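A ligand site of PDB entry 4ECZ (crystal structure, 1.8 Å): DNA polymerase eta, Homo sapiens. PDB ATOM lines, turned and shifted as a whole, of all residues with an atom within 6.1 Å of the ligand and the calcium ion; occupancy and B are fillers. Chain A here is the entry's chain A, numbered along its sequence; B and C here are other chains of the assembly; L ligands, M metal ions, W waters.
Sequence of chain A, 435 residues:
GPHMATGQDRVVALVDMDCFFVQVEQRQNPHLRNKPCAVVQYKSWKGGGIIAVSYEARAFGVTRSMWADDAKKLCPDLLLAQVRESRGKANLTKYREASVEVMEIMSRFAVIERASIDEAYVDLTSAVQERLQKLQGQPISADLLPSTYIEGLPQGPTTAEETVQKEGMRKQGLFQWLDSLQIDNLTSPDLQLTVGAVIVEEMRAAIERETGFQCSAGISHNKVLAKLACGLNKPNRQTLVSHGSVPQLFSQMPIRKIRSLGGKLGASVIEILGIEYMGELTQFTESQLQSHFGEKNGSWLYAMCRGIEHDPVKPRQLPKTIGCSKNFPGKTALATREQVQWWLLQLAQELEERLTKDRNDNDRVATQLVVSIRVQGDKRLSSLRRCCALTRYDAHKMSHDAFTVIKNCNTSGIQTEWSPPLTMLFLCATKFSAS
O4 of DT 4 of chain B is in hydrogen-bond range of N3 of the ligand, at 3.1 Å.
N of Phe 21 is in hydrogen-bond range of O12 of the ligand.
The side-chain hydroxyl (OH) of Tyr 55 is in hydrogen-bond range of an oxygen (O2) of the ligand (2.6 Å).
The guanidinium group (NH2) of Arg 64 lies within salt-bridge range of an oxygen (O5) of the ligand, 3.1 Å away.
The side-chain amino group of Lys 234 lies within salt-bridge range of an oxygen (O2) of the ligand (3.4 Å).
N of Cys 19 is in hydrogen-bond range of O2 of the ligand.
An oxygen (O1) of the ligand is in salt-bridge range of the guanidinium group of Arg 58 (3.2 Å).
N of Phe 20 lies within hydrogen-bond range of O12 of the ligand, 3.4 Å away.
OP2 of DT 8 of chain C lies within salt-bridge range of NZ of Lys 227, at 3.3 Å.
O3' of DT 8 of chain C is in hydrogen-bond range of the side-chain hydroxyl (OG) of Ser 116 (3.1 Å).
The side-chain carboxylate (OD1) of Asp 18 is in salt-bridge range of the side-chain amino group (NZ) of Lys 234 (2.7 Å).
The guanidinium group of Arg 58 sits at hydrogen-bond distance from the backbone carbonyl oxygen of Val 53.
NE2 of Gln 41 sits at hydrogen-bond distance from O2 of DT 4 of chain B, 2.7 Å away.
NE of Arg 64 sits at hydrogen-bond distance from O of Ile 51, at 2.9 Å.
O of Met 17 sits close to NZ of Lys 234.
The guanidinium group of Arg 58 lies close to the side-chain hydroxyl of Tyr 55.
O3' of DT 8 of chain C sits close to an oxygen (O8) of the ligand (3.4 Å).
Asp 18 touches the ligand.
O of Ile 51 touches C4 of the ligand, at 3.4 Å.
Ala 52 touches the ligand (CB to O12, 3.6 Å).
CG2 of Ile 117 touches O11 of the ligand, 3.9 Å away.
O4 of DT 3 of chain B touches N3 of the ligand, at 3.8 Å.
DA 5 of chain B touches the ligand (N1 to N4, 3.5 Å).
Hydrophobic or aromatic side chains within 4 Å of the ligand: Phe 20, Phe 21, Ile 51, Ala 52, Tyr 55 and Ile 117.
Of the 25 residues printed, 18 come within 4 Å of the ligand.
Three residues have an atom within 4 Å of the calcium ion: Asp 16, Met 17 and Asp 118.
Along chain A the residues within 4 Å of the calcium ion span positions 16 to 118.
The nearest printed residue that does not touch the calcium ion is Lys 234 (4.1 Å).
The calcium ion is bound by an oxygen (O4) of the ligand (2.3 Å).
The backbone carbonyl oxygen (O) of Met 17 binds the calcium ion (2.3 Å).
The calcium ion is bound by O3 of the ligand (2.4 Å).
The side-chain carboxylate (OD1) of Asp 118 binds the calcium ion (2.4 Å).
O8 of the ligand is bound to the calcium ion (2.4 Å).
OD1 of Asp 16 binds the calcium ion, at 2.7 Å.
The calcium ion is bound by OD2 of Asp 16.
Water W5 bridges a nitrogen (N2) of the ligand and the guanidinium group (NH1) of Arg 64.
Water W7 lies within hydrogen-bond range of NZ of Lys 227 (3.3 Å) and O7 of the ligand (3.5 Å).
Water W2 lies within hydrogen-bond range of O2 of DT 8 of chain C (2.7 Å) and an oxygen (O11) of the ligand (3.0 Å).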
ATOM      1  N   ASP A  16       1.817  -2.207 -16.986  1.00  0.00           N
ATOM      2  CA  ASP A  16       2.835  -1.538 -17.791  1.00  0.00           C
ATOM      3  C   ASP A  16       2.336  -1.181 -19.202  1.00  0.00           C
ATOM      4  O   ASP A  16       1.879  -2.031 -19.943  1.00  0.00           O
ATOM      5  CB  ASP A  16       4.070  -2.411 -17.900  1.00  0.00           C
ATOM      6  CG  ASP A  16       5.147  -1.764 -18.713  1.00  0.00           C
ATOM      7  OD1 ASP A  16       5.767  -2.465 -19.525  1.00  0.00           O
ATOM      8  OD2 ASP A  16       5.371  -0.547 -18.518  1.00  0.00           O
ATOM      9  N   MET A  17       2.457   0.096 -19.579  1.00  0.00           N
ATOM     10  CA  MET A  17       1.920   0.541 -20.872  1.00  0.00           C
ATOM     11  C   MET A  17       2.689  -0.118 -22.030  1.00  0.00           C
ATOM     12  O   MET A  17       3.890  -0.293 -21.952  1.00  0.00           O
ATOM     13  CB  MET A  17       1.974   2.070 -20.984  1.00  0.00           C
ATOM     14  CG  MET A  17       1.375   2.807 -19.783  1.00  0.00           C
ATOM     15  SD  MET A  17      -0.330   2.291 -19.442  1.00  0.00           S
ATOM     16  CE  MET A  17      -1.164   2.765 -20.926  1.00  0.00           C
ATOM     17  N   ASP A  18       1.990  -0.508 -23.084  1.00  0.00           N
ATOM     18  CA  ASP A  18       2.697  -1.056 -24.245  1.00  0.00           C
ATOM     19  C   ASP A  18       3.400   0.061 -25.024  1.00  0.00           C
ATOM     20  O   ASP A  18       2.837   1.139 -25.183  1.00  0.00           O
ATOM     21  CB  ASP A  18       1.713  -1.780 -25.171  1.00  0.00           C
ATOM     22  CG  ASP A  18       1.050  -2.969 -24.492  1.00  0.00           C
ATOM     23  OD1 ASP A  18       1.668  -3.583 -23.617  1.00  0.00           O
ATOM     24  OD2 ASP A  18      -0.107  -3.290 -24.838  1.00  0.00           O
ATOM     25  N   CYS A  19       4.608  -0.227 -25.530  1.00  0.00           N
ATOM     26  CA  CYS A  19       5.404   0.745 -26.297  1.00  0.00           C
ATOM     27  C   CYS A  19       4.974   2.182 -26.021  1.00  0.00           C
ATOM     28  O   CYS A  19       4.453   2.870 -26.899  1.00  0.00           O
ATOM     29  CB  CYS A  19       5.376   0.433 -27.806  1.00  0.00           C
ATOM     30  SG  CYS A  19       3.735   0.286 -28.558  1.00  0.00           S
ATOM     31  N   PHE A  20       5.205   2.634 -24.795  1.00  0.00           N
ATOM     32  CA  PHE A  20       4.490   3.795 -24.264  1.00  0.00           C
ATOM     33  C   PHE A  20       4.665   5.092 -25.058  1.00  0.00           C
ATOM     34  O   PHE A  20       3.675   5.673 -25.492  1.00  0.00           O
ATOM     35  CB  PHE A  20       4.813   4.019 -22.786  1.00  0.00           C
ATOM     36  CG  PHE A  20       4.067   5.160 -22.165  1.00  0.00           C
ATOM     37  CD1 PHE A  20       2.686   5.249 -22.259  1.00  0.00           C
ATOM     38  CD2 PHE A  20       4.749   6.158 -21.505  1.00  0.00           C
ATOM     39  CE1 PHE A  20       1.999   6.315 -21.689  1.00  0.00           C
ATOM     40  CE2 PHE A  20       4.074   7.222 -20.928  1.00  0.00           C
ATOM     41  CZ  PHE A  20       2.697   7.303 -21.016  1.00  0.00           C
ATOM     42  N   PHE A  21       5.901   5.537 -25.278  1.00  0.00           N
ATOM     43  CA  PHE A  21       6.081   6.808 -25.975  1.00  0.00           C
ATOM     44  C   PHE A  21       5.491   6.720 -27.402  1.00  0.00           C
ATOM     45  O   PHE A  21       4.971   7.706 -27.920  1.00  0.00           O
ATOM     46  CB  PHE A  21       7.546   7.272 -26.058  1.00  0.00           C
ATOM     47  CG  PHE A  21       8.138   7.703 -24.746  1.00  0.00           C
ATOM     48  CD1 PHE A  21       7.501   7.449 -23.542  1.00  0.00           C
ATOM     49  CD2 PHE A  21       9.366   8.365 -24.740  1.00  0.00           C
ATOM     50  CE1 PHE A  21       8.083   7.836 -22.335  1.00  0.00           C
ATOM     51  CE2 PHE A  21       9.949   8.768 -23.530  1.00  0.00           C
ATOM     52  CZ  PHE A  21       9.299   8.500 -22.336  1.00  0.00           C
ATOM     53  N   VAL A  22       5.590   5.540 -28.025  1.00  0.00           N
ATOM     54  CA  VAL A  22       4.972   5.357 -29.336  1.00  0.00           C
ATOM     55  C   VAL A  22       3.446   5.574 -29.276  1.00  0.00           C
ATOM     56  O   VAL A  22       2.860   6.285 -30.109  1.00  0.00           O
ATOM     57  CB  VAL A  22       5.310   3.974 -29.914  1.00  0.00           C
ATOM     58  CG1 VAL A  22       4.409   3.638 -31.102  1.00  0.00           C
ATOM     59  CG2 VAL A  22       6.798   3.902 -30.299  1.00  0.00           C
ATOM     60  N   GLN A  41      15.213  10.537 -30.451  1.00  0.00           N
ATOM     61  CA  GLN A  41      15.629  11.848 -29.952  1.00  0.00           C
ATOM     62  C   GLN A  41      16.826  12.340 -30.732  1.00  0.00           C
ATOM     63  O   GLN A  41      17.702  11.558 -31.104  1.00  0.00           O
ATOM     64  CB  GLN A  41      15.842  11.872 -28.432  1.00  0.00           C
ATOM     65  CG  GLN A  41      16.711  10.772 -27.874  1.00  0.00           C
ATOM     66  CD  GLN A  41      16.641  10.664 -26.350  1.00  0.00           C
ATOM     67  OE1 GLN A  41      15.817  11.306 -25.701  1.00  0.00           O
ATOM     68  NE2 GLN A  41      17.521   9.848 -25.784  1.00  0.00           N
ATOM     69  N   ILE A  51      14.194   5.452 -28.905  1.00  0.00           N
ATOM     70  CA  ILE A  51      13.872   5.177 -27.495  1.00  0.00           C
ATOM     71  C   ILE A  51      12.606   4.335 -27.254  1.00  0.00           C
ATOM     72  O   ILE A  51      12.379   3.845 -26.146  1.00  0.00           O
ATOM     73  CB  ILE A  51      13.842   6.478 -26.633  1.00  0.00           C
ATOM     74  CG1 ILE A  51      12.771   7.454 -27.127  1.00  0.00           C
ATOM     75  CG2 ILE A  51      15.215   7.154 -26.657  1.00  0.00           C
ATOM     76  CD1 ILE A  51      12.609   8.672 -26.208  1.00  0.00           C
ATOM     77  N   ALA A  52      11.796   4.159 -28.299  1.00  0.00           N
ATOM     78  CA  ALA A  52      10.569   3.356 -28.209  1.00  0.00           C
ATOM     79  C   ALA A  52      10.192   2.845 -29.596  1.00  0.00           C
ATOM     80  O   ALA A  52      10.376   3.552 -30.585  1.00  0.00           O
ATOM     81  CB  ALA A  52       9.435   4.185 -27.603  1.00  0.00           C
ATOM     82  N   VAL A  53       9.617   1.632 -29.652  1.00  0.00           N
ATOM     83  CA  VAL A  53       9.386   0.947 -30.929  1.00  0.00           C
ATOM     84  C   VAL A  53       8.034   0.235 -30.910  1.00  0.00           C
ATOM     85  O   VAL A  53       7.721  -0.501 -29.964  1.00  0.00           O
ATOM     86  CB  VAL A  53      10.485  -0.130 -31.175  1.00  0.00           C
ATOM     87  CG1 VAL A  53      10.342  -0.727 -32.559  1.00  0.00           C
ATOM     88  CG2 VAL A  53      11.835   0.470 -31.002  1.00  0.00           C
ATOM     89  N   TYR A  55       5.136  -2.463 -31.964  1.00  0.00           N
ATOM     90  CA  TYR A  55       5.233  -3.895 -32.170  1.00  0.00           C
ATOM     91  C   TYR A  55       5.339  -4.264 -33.654  1.00  0.00           C
ATOM     92  O   TYR A  55       6.030  -5.211 -34.017  1.00  0.00           O
ATOM     93  CB  TYR A  55       4.085  -4.607 -31.439  1.00  0.00           C
ATOM     94  CG  TYR A  55       4.355  -4.679 -29.943  1.00  0.00           C
ATOM     95  CD1 TYR A  55       4.109  -3.582 -29.113  1.00  0.00           C
ATOM     96  CD2 TYR A  55       4.930  -5.812 -29.377  1.00  0.00           C
ATOM     97  CE1 TYR A  55       4.407  -3.641 -27.742  1.00  0.00           C
ATOM     98  CE2 TYR A  55       5.223  -5.878 -28.029  1.00  0.00           C
ATOM     99  CZ  TYR A  55       4.963  -4.796 -27.208  1.00  0.00           C
ATOM    100  OH  TYR A  55       5.264  -4.875 -25.862  1.00  0.00           O
ATOM    101  N   ARG A  58       8.984  -3.846 -34.362  1.00  0.00           N
ATOM    102  CA  ARG A  58       9.799  -4.904 -33.730  1.00  0.00           C
ATOM    103  C   ARG A  58       9.878  -6.169 -34.593  1.00  0.00           C
ATOM    104  O   ARG A  58      10.903  -6.855 -34.591  1.00  0.00           O
ATOM    105  CB  ARG A  58       9.305  -5.260 -32.335  1.00  0.00           C
ATOM    106  CG  ARG A  58       9.315  -4.084 -31.395  1.00  0.00           C
ATOM    107  CD  ARG A  58       8.667  -4.439 -30.076  1.00  0.00           C
ATOM    108  NE  ARG A  58       8.441  -3.226 -29.302  1.00  0.00           N
ATOM    109  CZ  ARG A  58       8.181  -3.207 -27.995  1.00  0.00           C
ATOM    110  NH1 ARG A  58       8.119  -4.335 -27.312  1.00  0.00           N
ATOM    111  NH2 ARG A  58       7.983  -2.033 -27.390  1.00  0.00           N
ATOM    112  N   ARG A  64      15.202  -0.564 -29.363  1.00  0.00           N
ATOM    113  CA  ARG A  64      15.705   0.592 -28.625  1.00  0.00           C
ATOM    114  C   ARG A  64      17.240   0.670 -28.711  1.00  0.00           C
ATOM    115  O   ARG A  64      17.922  -0.358 -28.764  1.00  0.00           O
ATOM    116  CB  ARG A  64      15.223   0.491 -27.176  1.00  0.00           C
ATOM    117  CG  ARG A  64      15.864   1.462 -26.193  1.00  0.00           C
ATOM    118  CD  ARG A  64      15.194   1.318 -24.819  1.00  0.00           C
ATOM    119  NE  ARG A  64      13.783   1.683 -24.908  1.00  0.00           N
ATOM    120  CZ  ARG A  64      12.777   0.950 -24.432  1.00  0.00           C
ATOM    121  NH1 ARG A  64      13.009  -0.198 -23.814  1.00  0.00           N
ATOM    122  NH2 ARG A  64      11.529   1.384 -24.578  1.00  0.00           N
ATOM    123  N   SER A 116       7.894   3.552 -12.642  1.00  0.00           N
ATOM    124  CA  SER A 116       8.605   4.222 -13.727  1.00  0.00           C
ATOM    125  C   SER A 116       7.611   5.158 -14.416  1.00  0.00           C
ATOM    126  O   SER A 116       6.465   5.253 -14.010  1.00  0.00           O
ATOM    127  CB  SER A 116       9.122   3.186 -14.726  1.00  0.00           C
ATOM    128  OG  SER A 116       9.831   3.795 -15.797  1.00  0.00           O
ATOM    129  N   ILE A 117       8.034   5.822 -15.481  1.00  0.00           N
ATOM    130  CA  ILE A 117       7.122   6.700 -16.182  1.00  0.00           C
ATOM    131  C   ILE A 117       5.871   5.965 -16.697  1.00  0.00           C
ATOM    132  O   ILE A 117       4.822   6.582 -16.872  1.00  0.00           O
ATOM    133  CB  ILE A 117       7.820   7.428 -17.353  1.00  0.00           C
ATOM    134  CG1 ILE A 117       6.930   8.577 -17.862  1.00  0.00           C
ATOM    135  CG2 ILE A 117       8.148   6.458 -18.450  1.00  0.00           C
ATOM    136  CD1 ILE A 117       7.694   9.645 -18.632  1.00  0.00           C
ATOM    137  N   ASP A 118       5.962   4.646 -16.918  1.00  0.00           N
ATOM    138  CA  ASP A 118       4.803   3.961 -17.474  1.00  0.00           C
ATOM    139  C   ASP A 118       4.416   2.652 -16.788  1.00  0.00           C
ATOM    140  O   ASP A 118       3.735   1.807 -17.407  1.00  0.00           O
ATOM    141  CB  ASP A 118       4.985   3.702 -18.956  1.00  0.00           C
ATOM    142  CG  ASP A 118       5.816   2.471 -19.215  1.00  0.00           C
ATOM    143  OD1 ASP A 118       5.527   1.797 -20.214  1.00  0.00           O
ATOM    144  OD2 ASP A 118       6.722   2.153 -18.400  1.00  0.00           O
ATOM    145  N   GLU A 119       4.850   2.457 -15.545  1.00  0.00           N
ATOM    146  CA  GLU A 119       4.386   1.295 -14.814  1.00  0.00           C
ATOM    147  C   GLU A 119       4.098   1.603 -13.365  1.00  0.00           C
ATOM    148  O   GLU A 119       4.720   2.471 -12.752  1.00  0.00           O
ATOM    149  CB  GLU A 119       5.338   0.114 -14.956  1.00  0.00           C
ATOM    150  CG  GLU A 119       6.724   0.342 -14.422  1.00  0.00           C
ATOM    151  CD  GLU A 119       7.669  -0.754 -14.860  1.00  0.00           C
ATOM    152  OE1 GLU A 119       8.526  -0.483 -15.720  1.00  0.00           O
ATOM    153  OE2 GLU A 119       7.543  -1.885 -14.336  1.00  0.00           O
ATOM    154  N   LYS A 227       5.642  -8.573 -11.963  1.00  0.00           N
ATOM    155  CA  LYS A 227       6.475  -7.999 -13.028  1.00  0.00           C
ATOM    156  C   LYS A 227       6.865  -9.047 -14.069  1.00  0.00           C
ATOM    157  O   LYS A 227       6.711  -8.823 -15.286  1.00  0.00           O
ATOM    158  CB  LYS A 227       7.729  -7.345 -12.431  1.00  0.00           C
ATOM    159  CG  LYS A 227       8.759  -6.842 -13.456  1.00  0.00           C
ATOM    160  CD  LYS A 227       8.147  -5.834 -14.438  1.00  0.00           C
ATOM    161  CE  LYS A 227       9.243  -5.171 -15.291  1.00  0.00           C
ATOM    162  NZ  LYS A 227       8.672  -4.356 -16.396  1.00  0.00           N
ATOM    163  N   LYS A 234       2.781 -10.004 -23.866  1.00  0.00           N
ATOM    164  CA  LYS A 234       2.651  -8.606 -24.278  1.00  0.00           C
ATOM    165  C   LYS A 234       2.541  -8.670 -25.787  1.00  0.00           C
ATOM    166  O   LYS A 234       3.097  -9.579 -26.398  1.00  0.00           O
ATOM    167  CB  LYS A 234       3.929  -7.834 -23.893  1.00  0.00           C
ATOM    168  CG  LYS A 234       3.779  -6.864 -22.734  1.00  0.00           C
ATOM    169  CD  LYS A 234       4.953  -5.866 -22.709  1.00  0.00           C
ATOM    170  CE  LYS A 234       4.788  -4.817 -21.612  1.00  0.00           C
ATOM    171  NZ  LYS A 234       3.834  -3.706 -21.971  1.00  0.00           N
ATOM    172  N   PRO A 235       1.815  -7.711 -26.401  1.00  0.00           N
ATOM    173  CA  PRO A 235       1.126  -6.567 -25.792  1.00  0.00           C
ATOM    174  C   PRO A 235      -0.350  -6.816 -25.561  1.00  0.00           C
ATOM    175  O   PRO A 235      -0.913  -7.817 -26.004  1.00  0.00           O
ATOM    176  CB  PRO A 235       1.257  -5.487 -26.879  1.00  0.00           C
ATOM    177  CG  PRO A 235       1.159  -6.283 -28.158  1.00  0.00           C
ATOM    178  CD  PRO A 235       1.851  -7.612 -27.870  1.00  0.00           C
ATOM    179  P    DT B   3      27.719   4.651 -29.094  1.00  0.00           P
ATOM    180  OP1  DT B   3      29.144   4.333 -28.835  1.00  0.00           O
ATOM    181  OP2  DT B   3      26.924   3.842 -30.040  1.00  0.00           O
ATOM    182  O5'  DT B   3      26.975   4.650 -27.683  1.00  0.00           O
ATOM    183  C5'  DT B   3      25.560   4.445 -27.609  1.00  0.00           C
ATOM    184  C4'  DT B   3      24.848   5.774 -27.698  1.00  0.00           C
ATOM    185  O4'  DT B   3      23.415   5.582 -27.757  1.00  0.00           O
ATOM    186  C3'  DT B   3      25.062   6.688 -26.506  1.00  0.00           C
ATOM    187  O3'  DT B   3      25.023   7.998 -26.984  1.00  0.00           O
ATOM    188  C2'  DT B   3      23.874   6.402 -25.601  1.00  0.00           C
ATOM    189  C1'  DT B   3      22.779   6.175 -26.632  1.00  0.00           C
ATOM    190  N1   DT B   3      21.703   5.210 -26.216  1.00  0.00           N
ATOM    191  C2   DT B   3      20.382   5.545 -26.448  1.00  0.00           C
ATOM    192  O2   DT B   3      20.024   6.593 -26.969  1.00  0.00           O
ATOM    193  N3   DT B   3      19.472   4.595 -26.039  1.00  0.00           N
ATOM    194  C4   DT B   3      19.762   3.371 -25.458  1.00  0.00           C
ATOM    195  O4   DT B   3      18.866   2.594 -25.133  1.00  0.00           O
ATOM    196  C5   DT B   3      21.171   3.089 -25.244  1.00  0.00           C
ATOM    197  C7   DT B   3      21.623   1.796 -24.616  1.00  0.00           C
ATOM    198  C6   DT B   3      22.062   4.010 -25.643  1.00  0.00           C
ATOM    199  P    DT B   4      24.950   9.222 -25.948  1.00  0.00           P
ATOM    200  OP1  DT B   4      25.443  10.429 -26.644  1.00  0.00           O
ATOM    201  OP2  DT B   4      25.570   8.779 -24.680  1.00  0.00           O
ATOM    202  O5'  DT B   4      23.389   9.379 -25.668  1.00  0.00           O
ATOM    203  C5'  DT B   4      22.543  10.056 -26.592  1.00  0.00           C
ATOM    204  C4'  DT B   4      21.325  10.542 -25.847  1.00  0.00           C
ATOM    205  O4'  DT B   4      20.532   9.403 -25.422  1.00  0.00           O
ATOM    206  C3'  DT B   4      21.630  11.345 -24.589  1.00  0.00           C
ATOM    207  O3'  DT B   4      20.705  12.387 -24.613  1.00  0.00           O
ATOM    208  C2'  DT B   4      21.388  10.366 -23.443  1.00  0.00           C
ATOM    209  C1'  DT B   4      20.268   9.519 -24.040  1.00  0.00           C
ATOM    210  N1   DT B   4      20.151   8.132 -23.534  1.00  0.00           N
ATOM    211  C2   DT B   4      18.876   7.662 -23.367  1.00  0.00           C
ATOM    212  O2   DT B   4      17.886   8.330 -23.612  1.00  0.00           O
ATOM    213  N3   DT B   4      18.811   6.377 -22.918  1.00  0.00           N
ATOM    214  C4   DT B   4      19.857   5.537 -22.607  1.00  0.00           C
ATOM    215  O4   DT B   4      19.659   4.395 -22.216  1.00  0.00           O
ATOM    216  C5   DT B   4      21.181   6.088 -22.805  1.00  0.00           C
ATOM    217  C7   DT B   4      22.397   5.258 -22.510  1.00  0.00           C
ATOM    218  C6   DT B   4      21.261   7.349 -23.257  1.00  0.00           C
ATOM    219  P    DA B   5      20.637  13.449 -23.412  1.00  0.00           P
ATOM    220  OP1  DA B   5      20.325  14.751 -23.991  1.00  0.00           O
ATOM    221  OP2  DA B   5      21.847  13.262 -22.565  1.00  0.00           O
ATOM    222  O5'  DA B   5      19.416  12.941 -22.528  1.00  0.00           O
ATOM    223  C5'  DA B   5      18.074  13.013 -23.023  1.00  0.00           C
ATOM    224  C4'  DA B   5      17.082  12.616 -21.948  1.00  0.00           C
ATOM    225  O4'  DA B   5      17.174  11.189 -21.690  1.00  0.00           O
ATOM    226  C3'  DA B   5      17.267  13.309 -20.607  1.00  0.00           C
ATOM    227  O3'  DA B   5      15.994  13.647 -20.089  1.00  0.00           O
ATOM    228  C2'  DA B   5      17.962  12.241 -19.765  1.00  0.00           C
ATOM    229  C1'  DA B   5      17.284  10.970 -20.302  1.00  0.00           C
ATOM    230  N9   DA B   5      18.032   9.739 -20.093  1.00  0.00           N
ATOM    231  C8   DA B   5      19.391   9.559 -20.182  1.00  0.00           C
ATOM    232  N7   DA B   5      19.768   8.309 -19.958  1.00  0.00           N
ATOM    233  C5   DA B   5      18.588   7.639 -19.714  1.00  0.00           C
ATOM    234  C6   DA B   5      18.305   6.291 -19.393  1.00  0.00           C
ATOM    235  N6   DA B   5      19.266   5.376 -19.294  1.00  0.00           N
ATOM    236  N1   DA B   5      17.018   5.944 -19.212  1.00  0.00           N
ATOM    237  C2   DA B   5      16.080   6.884 -19.342  1.00  0.00           C
ATOM    238  N3   DA B   5      16.214   8.182 -19.624  1.00  0.00           N
ATOM    239  C4   DA B   5      17.510   8.494 -19.802  1.00  0.00           C
ATOM    240  P    DT C   8      12.605  -2.825 -15.244  1.00  0.00           P
ATOM    241  OP1  DT C   8      12.226  -2.699 -13.821  1.00  0.00           O
ATOM    242  OP2  DT C   8      11.894  -3.773 -16.134  1.00  0.00           O
ATOM    243  O5'  DT C   8      12.496  -1.392 -15.944  1.00  0.00           O
ATOM    244  C5'  DT C   8      11.453  -0.549 -15.512  1.00  0.00           C
ATOM    245  C4'  DT C   8      11.316   0.732 -16.332  1.00  0.00           C
ATOM    246  O4'  DT C   8      12.525   1.534 -16.351  1.00  0.00           O
ATOM    247  C3'  DT C   8      10.810   0.663 -17.782  1.00  0.00           C
ATOM    248  O3'  DT C   8       9.644   1.451 -17.881  1.00  0.00           O
ATOM    249  C2'  DT C   8      11.937   1.267 -18.620  1.00  0.00           C
ATOM    250  C1'  DT C   8      12.672   2.152 -17.624  1.00  0.00           C
ATOM    251  N1   DT C   8      14.133   2.276 -17.921  1.00  0.00           N
ATOM    252  C2   DT C   8      14.631   3.512 -18.256  1.00  0.00           C
ATOM    253  O2   DT C   8      13.944   4.508 -18.315  1.00  0.00           O
ATOM    254  N3   DT C   8      15.967   3.543 -18.512  1.00  0.00           N
ATOM    255  C4   DT C   8      16.850   2.491 -18.475  1.00  0.00           C
ATOM    256  O4   DT C   8      18.033   2.629 -18.722  1.00  0.00           O
ATOM    257  C5   DT C   8      16.263   1.211 -18.141  1.00  0.00           C
ATOM    258  C7   DT C   8      17.133  -0.009 -18.062  1.00  0.00           C
ATOM    259  C6   DT C   8      14.954   1.171 -17.879  1.00  0.00           C
HETATM  260  P1  LIG L   1       6.980  -2.395 -23.893  1.00  0.00           P
HETATM  261  O1  LIG L   1       7.964  -3.494 -24.245  1.00  0.00           O
HETATM  262  O2  LIG L   1       5.658  -2.584 -24.605  1.00  0.00           O
HETATM  263  O3  LIG L   1       6.897  -2.086 -22.424  1.00  0.00           O
HETATM  264  P2  LIG L   1       7.961   0.319 -23.850  1.00  0.00           P
HETATM  265  O4  LIG L   1       6.796   0.776 -23.007  1.00  0.00           O
HETATM  266  O5  LIG L   1       8.425   1.280 -24.927  1.00  0.00           O
HETATM  267  O6  LIG L   1       7.714  -1.109 -24.565  1.00  0.00           O
HETATM  268  P3  LIG L   1       9.553   0.270 -21.398  1.00  0.00           P
HETATM  269  O7  LIG L   1      10.901  -0.383 -21.119  1.00  0.00           O
HETATM  270  O8  LIG L   1       8.402  -0.153 -20.552  1.00  0.00           O
HETATM  271  O9  LIG L   1       9.284  -0.051 -22.980  1.00  0.00           O
HETATM  272  O10 LIG L   1       9.754   1.839 -21.244  1.00  0.00           O
HETATM  273  C1  LIG L   1       8.662   2.748 -21.155  1.00  0.00           C
HETATM  274  C2  LIG L   1       9.050   4.059 -21.855  1.00  0.00           C
HETATM  275  O11 LIG L   1      10.184   4.672 -21.223  1.00  0.00           O
HETATM  276  C3  LIG L   1       9.465   3.834 -23.311  1.00  0.00           C
HETATM  277  O12 LIG L   1       8.333   3.930 -24.189  1.00  0.00           O
HETATM  278  C4  LIG L   1      10.489   4.938 -23.548  1.00  0.00           C
HETATM  279  C5  LIG L   1      11.108   5.189 -22.179  1.00  0.00           C
HETATM  280  N1  LIG L   1      12.389   4.442 -22.078  1.00  0.00           N
HETATM  281  C6  LIG L   1      12.537   3.145 -21.738  1.00  0.00           C
HETATM  282  N2  LIG L   1      13.854   2.842 -21.751  1.00  0.00           N
HETATM  283  C7  LIG L   1      14.529   3.968 -22.081  1.00  0.00           C
HETATM  284  C8  LIG L   1      15.870   4.278 -22.237  1.00  0.00           C
HETATM  285  N3  LIG L   1      16.808   3.308 -22.060  1.00  0.00           N
HETATM  286  N4  LIG L   1      16.231   5.536 -22.602  1.00  0.00           N
HETATM  287  C9  LIG L   1      15.313   6.494 -22.787  1.00  0.00           C
HETATM  288  N5  LIG L   1      14.003   6.210 -22.634  1.00  0.00           N
HETATM  289  C10 LIG L   1      13.599   4.968 -22.275  1.00  0.00           C
HETATM  290 CA    CA M   1       6.074  -0.327 -21.100  1.00  0.00          CA
HETATM  291  O   HOH W   1      10.548  -3.302 -24.614  1.00  0.00           O
HETATM  292  O   HOH W   2      11.877   5.992 -19.131  1.00  0.00           O
HETATM  293  O   HOH W   3       9.810   0.464 -27.177  1.00  0.00           O
HETATM  294  O   HOH W   4       8.854  -4.322 -21.556  1.00  0.00           O
HETATM  295  O   HOH W   5      15.246   0.447 -21.362  1.00  0.00           O
HETATM  296  O   HOH W   6      12.900   8.698 -22.175  1.00  0.00           O
HETATM  297  O   HOH W   7       9.019  -2.477 -19.065  1.00  0.00           O
HETATM  298  O   HOH W   8      17.791   0.024 -22.103  1.00  0.00           O
